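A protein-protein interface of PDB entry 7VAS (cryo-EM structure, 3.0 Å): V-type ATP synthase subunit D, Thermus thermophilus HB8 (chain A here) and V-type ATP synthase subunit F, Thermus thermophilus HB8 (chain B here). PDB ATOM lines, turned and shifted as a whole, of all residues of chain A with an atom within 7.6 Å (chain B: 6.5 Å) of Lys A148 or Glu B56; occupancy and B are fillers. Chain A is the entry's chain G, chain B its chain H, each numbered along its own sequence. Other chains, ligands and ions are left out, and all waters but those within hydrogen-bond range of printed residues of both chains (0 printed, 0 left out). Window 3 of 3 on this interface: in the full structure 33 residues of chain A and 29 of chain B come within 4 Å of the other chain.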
ATOM      1  N   PHE A  39      15.100  32.866   5.952  1.00  0.00           N
ATOM      2  CA  PHE A  39      13.955  32.786   6.854  1.00  0.00           C
ATOM      3  C   PHE A  39      14.004  33.879   7.914  1.00  0.00           C
ATOM      4  O   PHE A  39      12.973  34.474   8.251  1.00  0.00           O
ATOM      5  CB  PHE A  39      13.918  31.405   7.508  1.00  0.00           C
ATOM      6  CG  PHE A  39      12.688  31.148   8.326  1.00  0.00           C
ATOM      7  CD1 PHE A  39      11.521  30.716   7.727  1.00  0.00           C
ATOM      8  CD2 PHE A  39      12.707  31.319   9.697  1.00  0.00           C
ATOM      9  CE1 PHE A  39      10.395  30.472   8.478  1.00  0.00           C
ATOM     10  CE2 PHE A  39      11.583  31.076  10.453  1.00  0.00           C
ATOM     11  CZ  PHE A  39      10.425  30.652   9.843  1.00  0.00           C
ATOM     12  N   LEU A  42      12.844  37.030   6.332  1.00  0.00           N
ATOM     13  CA  LEU A  42      11.409  37.035   6.076  1.00  0.00           C
ATOM     14  C   LEU A  42      10.596  37.197   7.356  1.00  0.00           C
ATOM     15  O   LEU A  42       9.499  37.759   7.317  1.00  0.00           O
ATOM     16  CB  LEU A  42      11.003  35.756   5.343  1.00  0.00           C
ATOM     17  CG  LEU A  42      10.925  35.839   3.817  1.00  0.00           C
ATOM     18  CD1 LEU A  42       9.815  36.786   3.398  1.00  0.00           C
ATOM     19  CD2 LEU A  42      12.249  36.273   3.215  1.00  0.00           C
ATOM     20  N   ARG A  50       2.733  42.911   9.507  1.00  0.00           N
ATOM     21  CA  ARG A  50       1.631  42.703  10.441  1.00  0.00           C
ATOM     22  C   ARG A  50       1.362  43.954  11.265  1.00  0.00           C
ATOM     23  O   ARG A  50       0.203  44.296  11.526  1.00  0.00           O
ATOM     24  CB  ARG A  50       1.933  41.515  11.352  1.00  0.00           C
ATOM     25  CG  ARG A  50       1.507  40.179  10.777  1.00  0.00           C
ATOM     26  CD  ARG A  50       0.050  39.893  11.074  1.00  0.00           C
ATOM     27  NE  ARG A  50      -0.448  38.756  10.312  1.00  0.00           N
ATOM     28  CZ  ARG A  50      -1.633  38.194  10.498  1.00  0.00           C
ATOM     29  NH1 ARG A  50      -2.469  38.635  11.424  1.00  0.00           N
ATOM     30  NH2 ARG A  50      -1.990  37.163   9.737  1.00  0.00           N
ATOM     31  N   VAL A 101       4.887  29.499  -5.658  1.00  0.00           N
ATOM     32  CA  VAL A 101       4.035  30.047  -4.612  1.00  0.00           C
ATOM     33  C   VAL A 101       3.123  31.090  -5.243  1.00  0.00           C
ATOM     34  O   VAL A 101       3.583  31.880  -6.070  1.00  0.00           O
ATOM     35  CB  VAL A 101       4.845  30.662  -3.454  1.00  0.00           C
ATOM     36  CG1 VAL A 101       5.713  31.813  -3.940  1.00  0.00           C
ATOM     37  CG2 VAL A 101       3.925  31.120  -2.339  1.00  0.00           C
ATOM     38  N   ALA A 141      -0.713  38.652   3.524  1.00  0.00           N
ATOM     39  CA  ALA A 141      -0.936  37.288   3.054  1.00  0.00           C
ATOM     40  C   ALA A 141       0.220  36.800   2.188  1.00  0.00           C
ATOM     41  O   ALA A 141       0.673  35.656   2.330  1.00  0.00           O
ATOM     42  CB  ALA A 141      -2.256  37.207   2.289  1.00  0.00           C
ATOM     43  N   ASN A 142       0.711  37.655   1.284  1.00  0.00           N
ATOM     44  CA  ASN A 142       1.837  37.270   0.435  1.00  0.00           C
ATOM     45  C   ASN A 142       3.068  36.936   1.266  1.00  0.00           C
ATOM     46  O   ASN A 142       3.728  35.907   1.049  1.00  0.00           O
ATOM     47  CB  ASN A 142       2.154  38.388  -0.556  1.00  0.00           C
ATOM     48  CG  ASN A 142       1.322  38.299  -1.809  1.00  0.00           C
ATOM     49  OD1 ASN A 142       0.663  37.290  -2.054  1.00  0.00           O
ATOM     50  ND2 ASN A 142       1.346  39.353  -2.614  1.00  0.00           N
ATOM     51  N   THR A 143       3.387  37.796   2.234  1.00  0.00           N
ATOM     52  CA  THR A 143       4.562  37.550   3.059  1.00  0.00           C
ATOM     53  C   THR A 143       4.408  36.263   3.861  1.00  0.00           C
ATOM     54  O   THR A 143       5.354  35.472   3.967  1.00  0.00           O
ATOM     55  CB  THR A 143       4.810  38.739   3.981  1.00  0.00           C
ATOM     56  OG1 THR A 143       4.955  39.924   3.192  1.00  0.00           O
ATOM     57  CG2 THR A 143       6.079  38.528   4.764  1.00  0.00           C
ATOM     58  N   GLU A 144       3.220  36.024   4.418  1.00  0.00           N
ATOM     59  CA  GLU A 144       3.013  34.807   5.194  1.00  0.00           C
ATOM     60  C   GLU A 144       3.165  33.567   4.325  1.00  0.00           C
ATOM     61  O   GLU A 144       3.724  32.555   4.767  1.00  0.00           O
ATOM     62  CB  GLU A 144       1.641  34.831   5.865  1.00  0.00           C
ATOM     63  CG  GLU A 144       1.598  35.664   7.130  1.00  0.00           C
ATOM     64  CD  GLU A 144       0.520  35.212   8.089  1.00  0.00           C
ATOM     65  OE1 GLU A 144       0.362  33.987   8.282  1.00  0.00           O
ATOM     66  OE2 GLU A 144      -0.173  36.087   8.646  1.00  0.00           O
ATOM     67  N   THR A 145       2.684  33.624   3.081  1.00  0.00           N
ATOM     68  CA  THR A 145       2.887  32.497   2.173  1.00  0.00           C
ATOM     69  C   THR A 145       4.369  32.256   1.920  1.00  0.00           C
ATOM     70  O   THR A 145       4.823  31.102   1.875  1.00  0.00           O
ATOM     71  CB  THR A 145       2.158  32.738   0.853  1.00  0.00           C
ATOM     72  OG1 THR A 145       2.444  34.060   0.383  1.00  0.00           O
ATOM     73  CG2 THR A 145       0.662  32.580   1.041  1.00  0.00           C
ATOM     74  N   ARG A 146       5.140  33.332   1.739  1.00  0.00           N
ATOM     75  CA  ARG A 146       6.574  33.166   1.509  1.00  0.00           C
ATOM     76  C   ARG A 146       7.254  32.496   2.702  1.00  0.00           C
ATOM     77  O   ARG A 146       8.057  31.565   2.534  1.00  0.00           O
ATOM     78  CB  ARG A 146       7.221  34.515   1.208  1.00  0.00           C
ATOM     79  CG  ARG A 146       7.174  34.905  -0.254  1.00  0.00           C
ATOM     80  CD  ARG A 146       8.299  35.860  -0.601  1.00  0.00           C
ATOM     81  NE  ARG A 146       9.599  35.202  -0.530  1.00  0.00           N
ATOM     82  CZ  ARG A 146      10.756  35.800  -0.775  1.00  0.00           C
ATOM     83  NH1 ARG A 146      10.818  37.077  -1.112  1.00  0.00           N
ATOM     84  NH2 ARG A 146      11.881  35.097  -0.682  1.00  0.00           N
ATOM     85  N   LEU A 147       6.945  32.958   3.919  1.00  0.00           N
ATOM     86  CA  LEU A 147       7.513  32.315   5.105  1.00  0.00           C
ATOM     87  C   LEU A 147       7.100  30.855   5.213  1.00  0.00           C
ATOM     88  O   LEU A 147       7.910  30.009   5.601  1.00  0.00           O
ATOM     89  CB  LEU A 147       7.146  33.058   6.392  1.00  0.00           C
ATOM     90  CG  LEU A 147       7.889  34.336   6.783  1.00  0.00           C
ATOM     91  CD1 LEU A 147       7.550  35.515   5.918  1.00  0.00           C
ATOM     92  CD2 LEU A 147       7.627  34.646   8.254  1.00  0.00           C
ATOM     93  N   LYS A 148       5.845  30.538   4.895  1.00  0.00           N
ATOM     94  CA  LYS A 148       5.417  29.143   4.957  1.00  0.00           C
ATOM     95  C   LYS A 148       6.215  28.273   3.993  1.00  0.00           C
ATOM     96  O   LYS A 148       6.658  27.175   4.357  1.00  0.00           O
ATOM     97  CB  LYS A 148       3.923  29.039   4.668  1.00  0.00           C
ATOM     98  CG  LYS A 148       3.052  29.537   5.800  1.00  0.00           C
ATOM     99  CD  LYS A 148       1.582  29.417   5.461  1.00  0.00           C
ATOM    100  CE  LYS A 148       0.734  29.437   6.716  1.00  0.00           C
ATOM    101  NZ  LYS A 148       0.769  30.769   7.374  1.00  0.00           N
ATOM    102  N   LYS A 149       6.419  28.749   2.763  1.00  0.00           N
ATOM    103  CA  LYS A 149       7.195  27.973   1.799  1.00  0.00           C
ATOM    104  C   LYS A 149       8.632  27.772   2.271  1.00  0.00           C
ATOM    105  O   LYS A 149       9.174  26.657   2.194  1.00  0.00           O
ATOM    106  CB  LYS A 149       7.171  28.657   0.433  1.00  0.00           C
ATOM    107  CG  LYS A 149       5.986  28.274  -0.435  1.00  0.00           C
ATOM    108  CD  LYS A 149       6.002  26.795  -0.780  1.00  0.00           C
ATOM    109  CE  LYS A 149       4.907  26.453  -1.781  1.00  0.00           C
ATOM    110  NZ  LYS A 149       4.852  24.997  -2.083  1.00  0.00           N
ATOM    111  N   ILE A 150       9.265  28.836   2.773  1.00  0.00           N
ATOM    112  CA  ILE A 150      10.650  28.715   3.224  1.00  0.00           C
ATOM    113  C   ILE A 150      10.744  27.761   4.410  1.00  0.00           C
ATOM    114  O   ILE A 150      11.692  26.973   4.521  1.00  0.00           O
ATOM    115  CB  ILE A 150      11.227  30.102   3.558  1.00  0.00           C
ATOM    116  CG1 ILE A 150      11.344  30.940   2.287  1.00  0.00           C
ATOM    117  CG2 ILE A 150      12.588  29.973   4.216  1.00  0.00           C
ATOM    118  CD1 ILE A 150      12.314  30.381   1.281  1.00  0.00           C
ATOM    119  N   GLY A 151       9.759  27.807   5.308  1.00  0.00           N
ATOM    120  CA  GLY A 151       9.753  26.887   6.431  1.00  0.00           C
ATOM    121  C   GLY A 151       9.606  25.440   6.002  1.00  0.00           C
ATOM    122  O   GLY A 151      10.253  24.550   6.558  1.00  0.00           O
ATOM    123  N   GLU A 152       8.747  25.186   5.011  1.00  0.00           N
ATOM    124  CA  GLU A 152       8.616  23.824   4.497  1.00  0.00           C
ATOM    125  C   GLU A 152       9.929  23.338   3.901  1.00  0.00           C
ATOM    126  O   GLU A 152      10.331  22.185   4.113  1.00  0.00           O
ATOM    127  CB  GLU A 152       7.498  23.749   3.459  1.00  0.00           C
ATOM    128  CG  GLU A 152       6.116  24.084   3.993  1.00  0.00           C
ATOM    129  CD  GLU A 152       5.859  23.508   5.374  1.00  0.00           C
ATOM    130  OE1 GLU A 152       6.090  22.297   5.572  1.00  0.00           O
ATOM    131  OE2 GLU A 152       5.423  24.270   6.261  1.00  0.00           O
ATOM    132  N   GLU A 153      10.618  24.207   3.158  1.00  0.00           N
ATOM    133  CA  GLU A 153      11.911  23.818   2.598  1.00  0.00           C
ATOM    134  C   GLU A 153      12.923  23.510   3.697  1.00  0.00           C
ATOM    135  O   GLU A 153      13.680  22.535   3.601  1.00  0.00           O
ATOM    136  CB  GLU A 153      12.435  24.917   1.677  1.00  0.00           C
ATOM    137  CG  GLU A 153      11.702  24.996   0.357  1.00  0.00           C
ATOM    138  CD  GLU A 153      11.893  23.749  -0.479  1.00  0.00           C
ATOM    139  OE1 GLU A 153      13.057  23.395  -0.758  1.00  0.00           O
ATOM    140  OE2 GLU A 153      10.880  23.120  -0.852  1.00  0.00           O
ATOM    141  N   ILE A 154      12.947  24.330   4.750  1.00  0.00           N
ATOM    142  CA  ILE A 154      13.882  24.101   5.849  1.00  0.00           C
ATOM    143  C   ILE A 154      13.588  22.773   6.534  1.00  0.00           C
ATOM    144  O   ILE A 154      14.506  22.005   6.856  1.00  0.00           O
ATOM    145  CB  ILE A 154      13.832  25.273   6.845  1.00  0.00           C
ATOM    146  CG1 ILE A 154      14.622  26.462   6.304  1.00  0.00           C
ATOM    147  CG2 ILE A 154      14.378  24.854   8.196  1.00  0.00           C
ATOM    148  CD1 ILE A 154      14.370  27.745   7.047  1.00  0.00           C
ATOM    149  N   LEU B  33     -16.901  28.944   6.343  1.00  0.00           N
ATOM    150  CA  LEU B  33     -15.649  28.759   5.618  1.00  0.00           C
ATOM    151  C   LEU B  33     -15.683  27.492   4.774  1.00  0.00           C
ATOM    152  O   LEU B  33     -15.208  27.483   3.631  1.00  0.00           O
ATOM    153  CB  LEU B  33     -14.482  28.720   6.605  1.00  0.00           C
ATOM    154  CG  LEU B  33     -13.143  28.193   6.093  1.00  0.00           C
ATOM    155  CD1 LEU B  33     -12.571  29.127   5.041  1.00  0.00           C
ATOM    156  CD2 LEU B  33     -12.168  28.015   7.245  1.00  0.00           C
ATOM    157  N   ASP B  54      -6.735  29.082  13.588  1.00  0.00           N
ATOM    158  CA  ASP B  54      -5.969  28.606  12.436  1.00  0.00           C
ATOM    159  C   ASP B  54      -6.953  28.255  11.329  1.00  0.00           C
ATOM    160  O   ASP B  54      -7.482  27.132  11.287  1.00  0.00           O
ATOM    161  CB  ASP B  54      -5.098  27.408  12.808  1.00  0.00           C
ATOM    162  CG  ASP B  54      -3.964  27.781  13.743  1.00  0.00           C
ATOM    163  OD1 ASP B  54      -3.641  28.985  13.841  1.00  0.00           O
ATOM    164  OD2 ASP B  54      -3.392  26.871  14.380  1.00  0.00           O
ATOM    165  N   PRO B  55      -7.235  29.189  10.416  1.00  0.00           N
ATOM    166  CA  PRO B  55      -8.253  28.922   9.385  1.00  0.00           C
ATOM    167  C   PRO B  55      -7.943  27.715   8.516  1.00  0.00           C
ATOM    168  O   PRO B  55      -8.864  26.993   8.116  1.00  0.00           O
ATOM    169  CB  PRO B  55      -8.264  30.221   8.567  1.00  0.00           C
ATOM    170  CG  PRO B  55      -7.727  31.260   9.499  1.00  0.00           C
ATOM    171  CD  PRO B  55      -6.701  30.557  10.330  1.00  0.00           C
ATOM    172  N   GLU B  56      -6.667  27.475   8.211  1.00  0.00           N
ATOM    173  CA  GLU B  56      -6.319  26.330   7.378  1.00  0.00           C
ATOM    174  C   GLU B  56      -6.466  25.016   8.134  1.00  0.00           C
ATOM    175  O   GLU B  56      -6.697  23.972   7.515  1.00  0.00           O
ATOM    176  CB  GLU B  56      -4.897  26.481   6.842  1.00  0.00           C
ATOM    177  CG  GLU B  56      -3.844  26.668   7.919  1.00  0.00           C
ATOM    178  CD  GLU B  56      -2.543  27.212   7.367  1.00  0.00           C
ATOM    179  OE1 GLU B  56      -2.006  26.619   6.408  1.00  0.00           O
ATOM    180  OE2 GLU B  56      -2.056  28.236   7.892  1.00  0.00           O
ATOM    181  N   ARG B  57      -6.331  25.042   9.461  1.00  0.00           N
ATOM    182  CA  ARG B  57      -6.453  23.812  10.238  1.00  0.00           C
ATOM    183  C   ARG B  57      -7.853  23.223  10.131  1.00  0.00           C
ATOM    184  O   ARG B  57      -8.015  22.003  10.013  1.00  0.00           O
ATOM    185  CB  ARG B  57      -6.093  24.075  11.699  1.00  0.00           C
ATOM    186  CG  ARG B  57      -6.022  22.821  12.552  1.00  0.00           C
ATOM    187  CD  ARG B  57      -5.638  23.148  13.985  1.00  0.00           C
ATOM    188  NE  ARG B  57      -4.359  23.845  14.060  1.00  0.00           N
ATOM    189  CZ  ARG B  57      -3.190  23.250  14.251  1.00  0.00           C
ATOM    190  NH1 ARG B  57      -3.095  21.938  14.397  1.00  0.00           N
ATOM    191  NH2 ARG B  57      -2.085  23.991  14.299  1.00  0.00           N
ATOM    192  N   ALA B  58      -8.879  24.076  10.170  1.00  0.00           N
ATOM    193  CA  ALA B  58     -10.255  23.590  10.168  1.00  0.00           C
ATOM    194  C   ALA B  58     -10.622  22.908   8.856  1.00  0.00           C
ATOM    195  O   ALA B  58     -11.370  21.924   8.863  1.00  0.00           O
ATOM    196  CB  ALA B  58     -11.217  24.742  10.454  1.00  0.00           C
ATOM    197  N   VAL B  59     -10.118  23.407   7.730  1.00  0.00           N
ATOM    198  CA  VAL B  59     -10.463  22.852   6.425  1.00  0.00           C
ATOM    199  C   VAL B  59      -9.222  22.243   5.789  1.00  0.00           C
ATOM    200  O   VAL B  59      -9.088  22.211   4.561  1.00  0.00           O
ATOM    201  CB  VAL B  59     -11.090  23.923   5.514  1.00  0.00           C
ATOM    202  CG1 VAL B  59     -12.398  24.411   6.107  1.00  0.00           C
ATOM    203  CG2 VAL B  59     -10.131  25.087   5.319  1.00  0.00           C
ATOM    204  N   GLU B  60      -8.310  21.748   6.630  1.00  0.00           N
ATOM    205  CA  GLU B  60      -7.059  21.183   6.139  1.00  0.00           C
ATOM    206  C   GLU B  60      -7.300  20.006   5.202  1.00  0.00           C
ATOM    207  O   GLU B  60      -6.640  19.886   4.163  1.00  0.00           O
ATOM    208  CB  GLU B  60      -6.188  20.759   7.323  1.00  0.00           C
ATOM    209  CG  GLU B  60      -4.849  20.161   6.939  1.00  0.00           C
ATOM    210  CD  GLU B  60      -4.044  19.725   8.149  1.00  0.00           C
ATOM    211  OE1 GLU B  60      -4.620  19.064   9.039  1.00  0.00           O
ATOM    212  OE2 GLU B  60      -2.838  20.042   8.210  1.00  0.00           O
ATOM    213  N   ARG B  61      -8.236  19.122   5.552  1.00  0.00           N
ATOM    214  CA  ARG B  61      -8.524  17.979   4.694  1.00  0.00           C
ATOM    215  C   ARG B  61      -9.088  18.421   3.350  1.00  0.00           C
ATOM    216  O   ARG B  61      -8.690  17.905   2.299  1.00  0.00           O
ATOM    217  CB  ARG B  61      -9.489  17.023   5.394  1.00  0.00           C
ATOM    218  CG  ARG B  61      -9.702  15.711   4.660  1.00  0.00           C
ATOM    219  CD  ARG B  61      -8.376  15.071   4.285  1.00  0.00           C
ATOM    220  NE  ARG B  61      -7.590  14.715   5.461  1.00  0.00           N
ATOM    221  CZ  ARG B  61      -7.221  13.480   5.769  1.00  0.00           C
ATOM    222  NH1 ARG B  61      -7.554  12.450   5.008  1.00  0.00           N
ATOM    223  NH2 ARG B  61      -6.499  13.273   6.866  1.00  0.00           N
ATOM    224  N   MET B  63      -8.614  21.274   1.959  1.00  0.00           N
ATOM    225  CA  MET B  63      -7.613  22.095   1.291  1.00  0.00           C
ATOM    226  C   MET B  63      -6.427  21.291   0.774  1.00  0.00           C
ATOM    227  O   MET B  63      -5.378  21.882   0.490  1.00  0.00           O
ATOM    228  CB  MET B  63      -7.121  23.197   2.233  1.00  0.00           C
ATOM    229  CG  MET B  63      -8.047  24.397   2.327  1.00  0.00           C
ATOM    230  SD  MET B  63      -7.999  25.442   0.858  1.00  0.00           S
ATOM    231  CE  MET B  63      -9.605  25.102   0.143  1.00  0.00           C
ATOM    232  N   LEU B  71      -5.620  31.178   3.186  1.00  0.00           N
ATOM    233  CA  LEU B  71      -6.389  31.450   4.392  1.00  0.00           C
ATOM    234  C   LEU B  71      -5.481  32.070   5.443  1.00  0.00           C
ATOM    235  O   LEU B  71      -4.377  31.572   5.687  1.00  0.00           O
ATOM    236  CB  LEU B  71      -7.024  30.167   4.939  1.00  0.00           C
ATOM    237  CG  LEU B  71      -8.461  29.839   4.528  1.00  0.00           C
ATOM    238  CD1 LEU B  71      -8.588  29.684   3.021  1.00  0.00           C
ATOM    239  CD2 LEU B  71      -8.925  28.579   5.231  1.00  0.00           C
ATOM    240  N   LEU B  72      -5.944  33.150   6.064  1.00  0.00           N
ATOM    241  CA  LEU B  72      -5.213  33.802   7.138  1.00  0.00           C
ATOM    242  C   LEU B  72      -6.194  34.335   8.169  1.00  0.00           C
ATOM    243  O   LEU B  72      -7.331  34.682   7.828  1.00  0.00           O
ATOM    244  CB  LEU B  72      -4.333  34.953   6.619  1.00  0.00           C
ATOM    245  CG  LEU B  72      -4.993  36.257   6.163  1.00  0.00           C
ATOM    246  CD1 LEU B  72      -3.949  37.354   6.059  1.00  0.00           C
ATOM    247  CD2 LEU B  72      -5.706  36.083   4.835  1.00  0.00           C
ATOM    248  N   PRO B  73      -5.790  34.404   9.436  1.00  0.00           N
ATOM    249  CA  PRO B  73      -6.660  34.962  10.471  1.00  0.00           C
ATOM    250  C   PRO B  73      -6.484  36.463  10.639  1.00  0.00           C
ATOM    251  O   PRO B  73      -5.419  37.030  10.389  1.00  0.00           O
ATOM    252  CB  PRO B  73      -6.202  34.216  11.732  1.00  0.00           C
ATOM    253  CG  PRO B  73      -4.753  33.979  11.495  1.00  0.00           C
ATOM    254  CD  PRO B  73      -4.578  33.789  10.006  1.00  0.00           C
ATOM    255  N   TYR B  89       1.806  35.947  18.151  1.00  0.00           N
ATOM    256  CA  TYR B  89       1.427  35.335  16.882  1.00  0.00           C
ATOM    257  C   TYR B  89       2.654  34.935  16.076  1.00  0.00           C
ATOM    258  O   TYR B  89       2.702  33.838  15.505  1.00  0.00           O
ATOM    259  CB  TYR B  89       0.548  36.297  16.082  1.00  0.00           C
ATOM    260  CG  TYR B  89       0.235  35.821  14.684  1.00  0.00           C
ATOM    261  CD1 TYR B  89      -0.679  34.800  14.467  1.00  0.00           C
ATOM    262  CD2 TYR B  89       0.855  36.390  13.583  1.00  0.00           C
ATOM    263  CE1 TYR B  89      -0.969  34.360  13.192  1.00  0.00           C
ATOM    264  CE2 TYR B  89       0.572  35.958  12.302  1.00  0.00           C
ATOM    265  CZ  TYR B  89      -0.340  34.943  12.114  1.00  0.00           C
ATOM    266  OH  TYR B  89      -0.625  34.507  10.842  1.00  0.00           O
ATOM    267  N   LEU B  93       3.791  31.192  14.992  1.00  0.00           N
ATOM    268  CA  LEU B  93       4.036  30.869  13.590  1.00  0.00           C
ATOM    269  C   LEU B  93       5.424  30.271  13.392  1.00  0.00           C
ATOM    270  O   LEU B  93       5.588  29.294  12.652  1.00  0.00           O
ATOM    271  CB  LEU B  93       3.862  32.121  12.732  1.00  0.00           C
ATOM    272  CG  LEU B  93       4.149  31.977  11.239  1.00  0.00           C
ATOM    273  CD1 LEU B  93       3.112  31.083  10.581  1.00  0.00           C
ATOM    274  CD2 LEU B  93       4.182  33.343  10.579  1.00  0.00           C
ATOM    275  N   LYS B  96       5.453  26.737  14.732  1.00  0.00           N
ATOM    276  CA  LYS B  96       4.803  25.806  13.817  1.00  0.00           C
ATOM    277  C   LYS B  96       5.675  25.514  12.602  1.00  0.00           C
ATOM    278  O   LYS B  96       5.780  24.360  12.169  1.00  0.00           O
ATOM    279  CB  LYS B  96       3.447  26.357  13.381  1.00  0.00           C
ATOM    280  CG  LYS B  96       2.388  26.314  14.461  1.00  0.00           C
ATOM    281  CD  LYS B  96       1.012  26.549  13.874  1.00  0.00           C
ATOM    282  CE  LYS B  96       0.681  25.480  12.849  1.00  0.00           C
ATOM    283  NZ  LYS B  96       0.828  24.115  13.424  1.00  0.00           N
ATOM    284  N   THR B  97       6.306  26.544  12.036  1.00  0.00           N
ATOM    285  CA  THR B  97       7.047  26.363  10.791  1.00  0.00           C
ATOM    286  C   THR B  97       8.348  25.601  11.014  1.00  0.00           C
ATOM    287  O   THR B  97       8.680  24.686  10.253  1.00  0.00           O
ATOM    288  CB  THR B  97       7.330  27.722  10.148  1.00  0.00           C
ATOM    289  OG1 THR B  97       7.807  28.631  11.147  1.00  0.00           O
ATOM    290  CG2 THR B  97       6.068  28.286   9.524  1.00  0.00           C
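The guanidinium group of Arg A50 lies within salt-bridge range of the side-chain carboxylate of Glu A144, 3.2 Å away.
OE1 of Glu A144 is in salt-bridge range of NZ of Lys A148 (3.4 Å).
OG1 of Thr B97 is in hydrogen-bond range of O of Leu B93, 2.8 Å away.
Printed residues of chain B within 4 Å of Lys A148: Glu B56 (3.3 Å) and Leu B93 (3.98 Å).
Of chain A, only Lys A148 comes within 4 Å of Glu B56.
Of the printed residues of chain A, Leu B93 touches Lys A148 (3.98 Å).
Printed residues of chain B within 4 Å of Glu A144: Tyr B89 (2.7 Å).
Printed residues of chain A within 4 Å of Tyr B89: Arg A50 (3.2 Å) and Glu A144 (2.7 Å).
Printed residues of chain B within 4 Å of Arg A50: Pro B73 (3.5 Å) and Tyr B89 (3.2 Å).
Of the printed residues of chain A, Pro B73 touches Arg A50.
The nearest printed residue of chain B that does not touch Lys A148 is Thr B97 (4.7 Å).
The nearest residue of chain A that does not touch Glu B56 is Glu A144 (6.3 Å).
The backbone carbonyl oxygen (O) of Pro B73 lies within hydrogen-bond range of the guanidinium group (NH2) of Arg A50 (3.5 Å).
The side-chain hydroxyl of Tyr B89 is in hydrogen-bond range of the guanidinium group of Arg A50 (3.2 Å).
OH of Tyr B89 is in hydrogen-bond range of OE2 of Glu A144, at 2.7 Å.
The side-chain carboxylate (OE2) of Glu B56 lies within salt-bridge range of the side-chain amino group (NZ) of Lys A148 (3.8 Å).
OG1 of Thr B97 touches CZ of Phe A39, at 3.6 Å.
Lys A148 touches Leu B93 (NZ to CD1, 3.98 Å).
Of the 17 printed residues of chain B, 5 touch a printed residue of chain A.
Of the 18 printed residues of chain A, 4 touch a printed residue of chain B.
Among the printed residues, Asp or Glu carboxylates within 4 Å of a Lys or Arg side-chain nitrogen of the other chain: Lys A148 with Glu B56 (3.8 Å).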
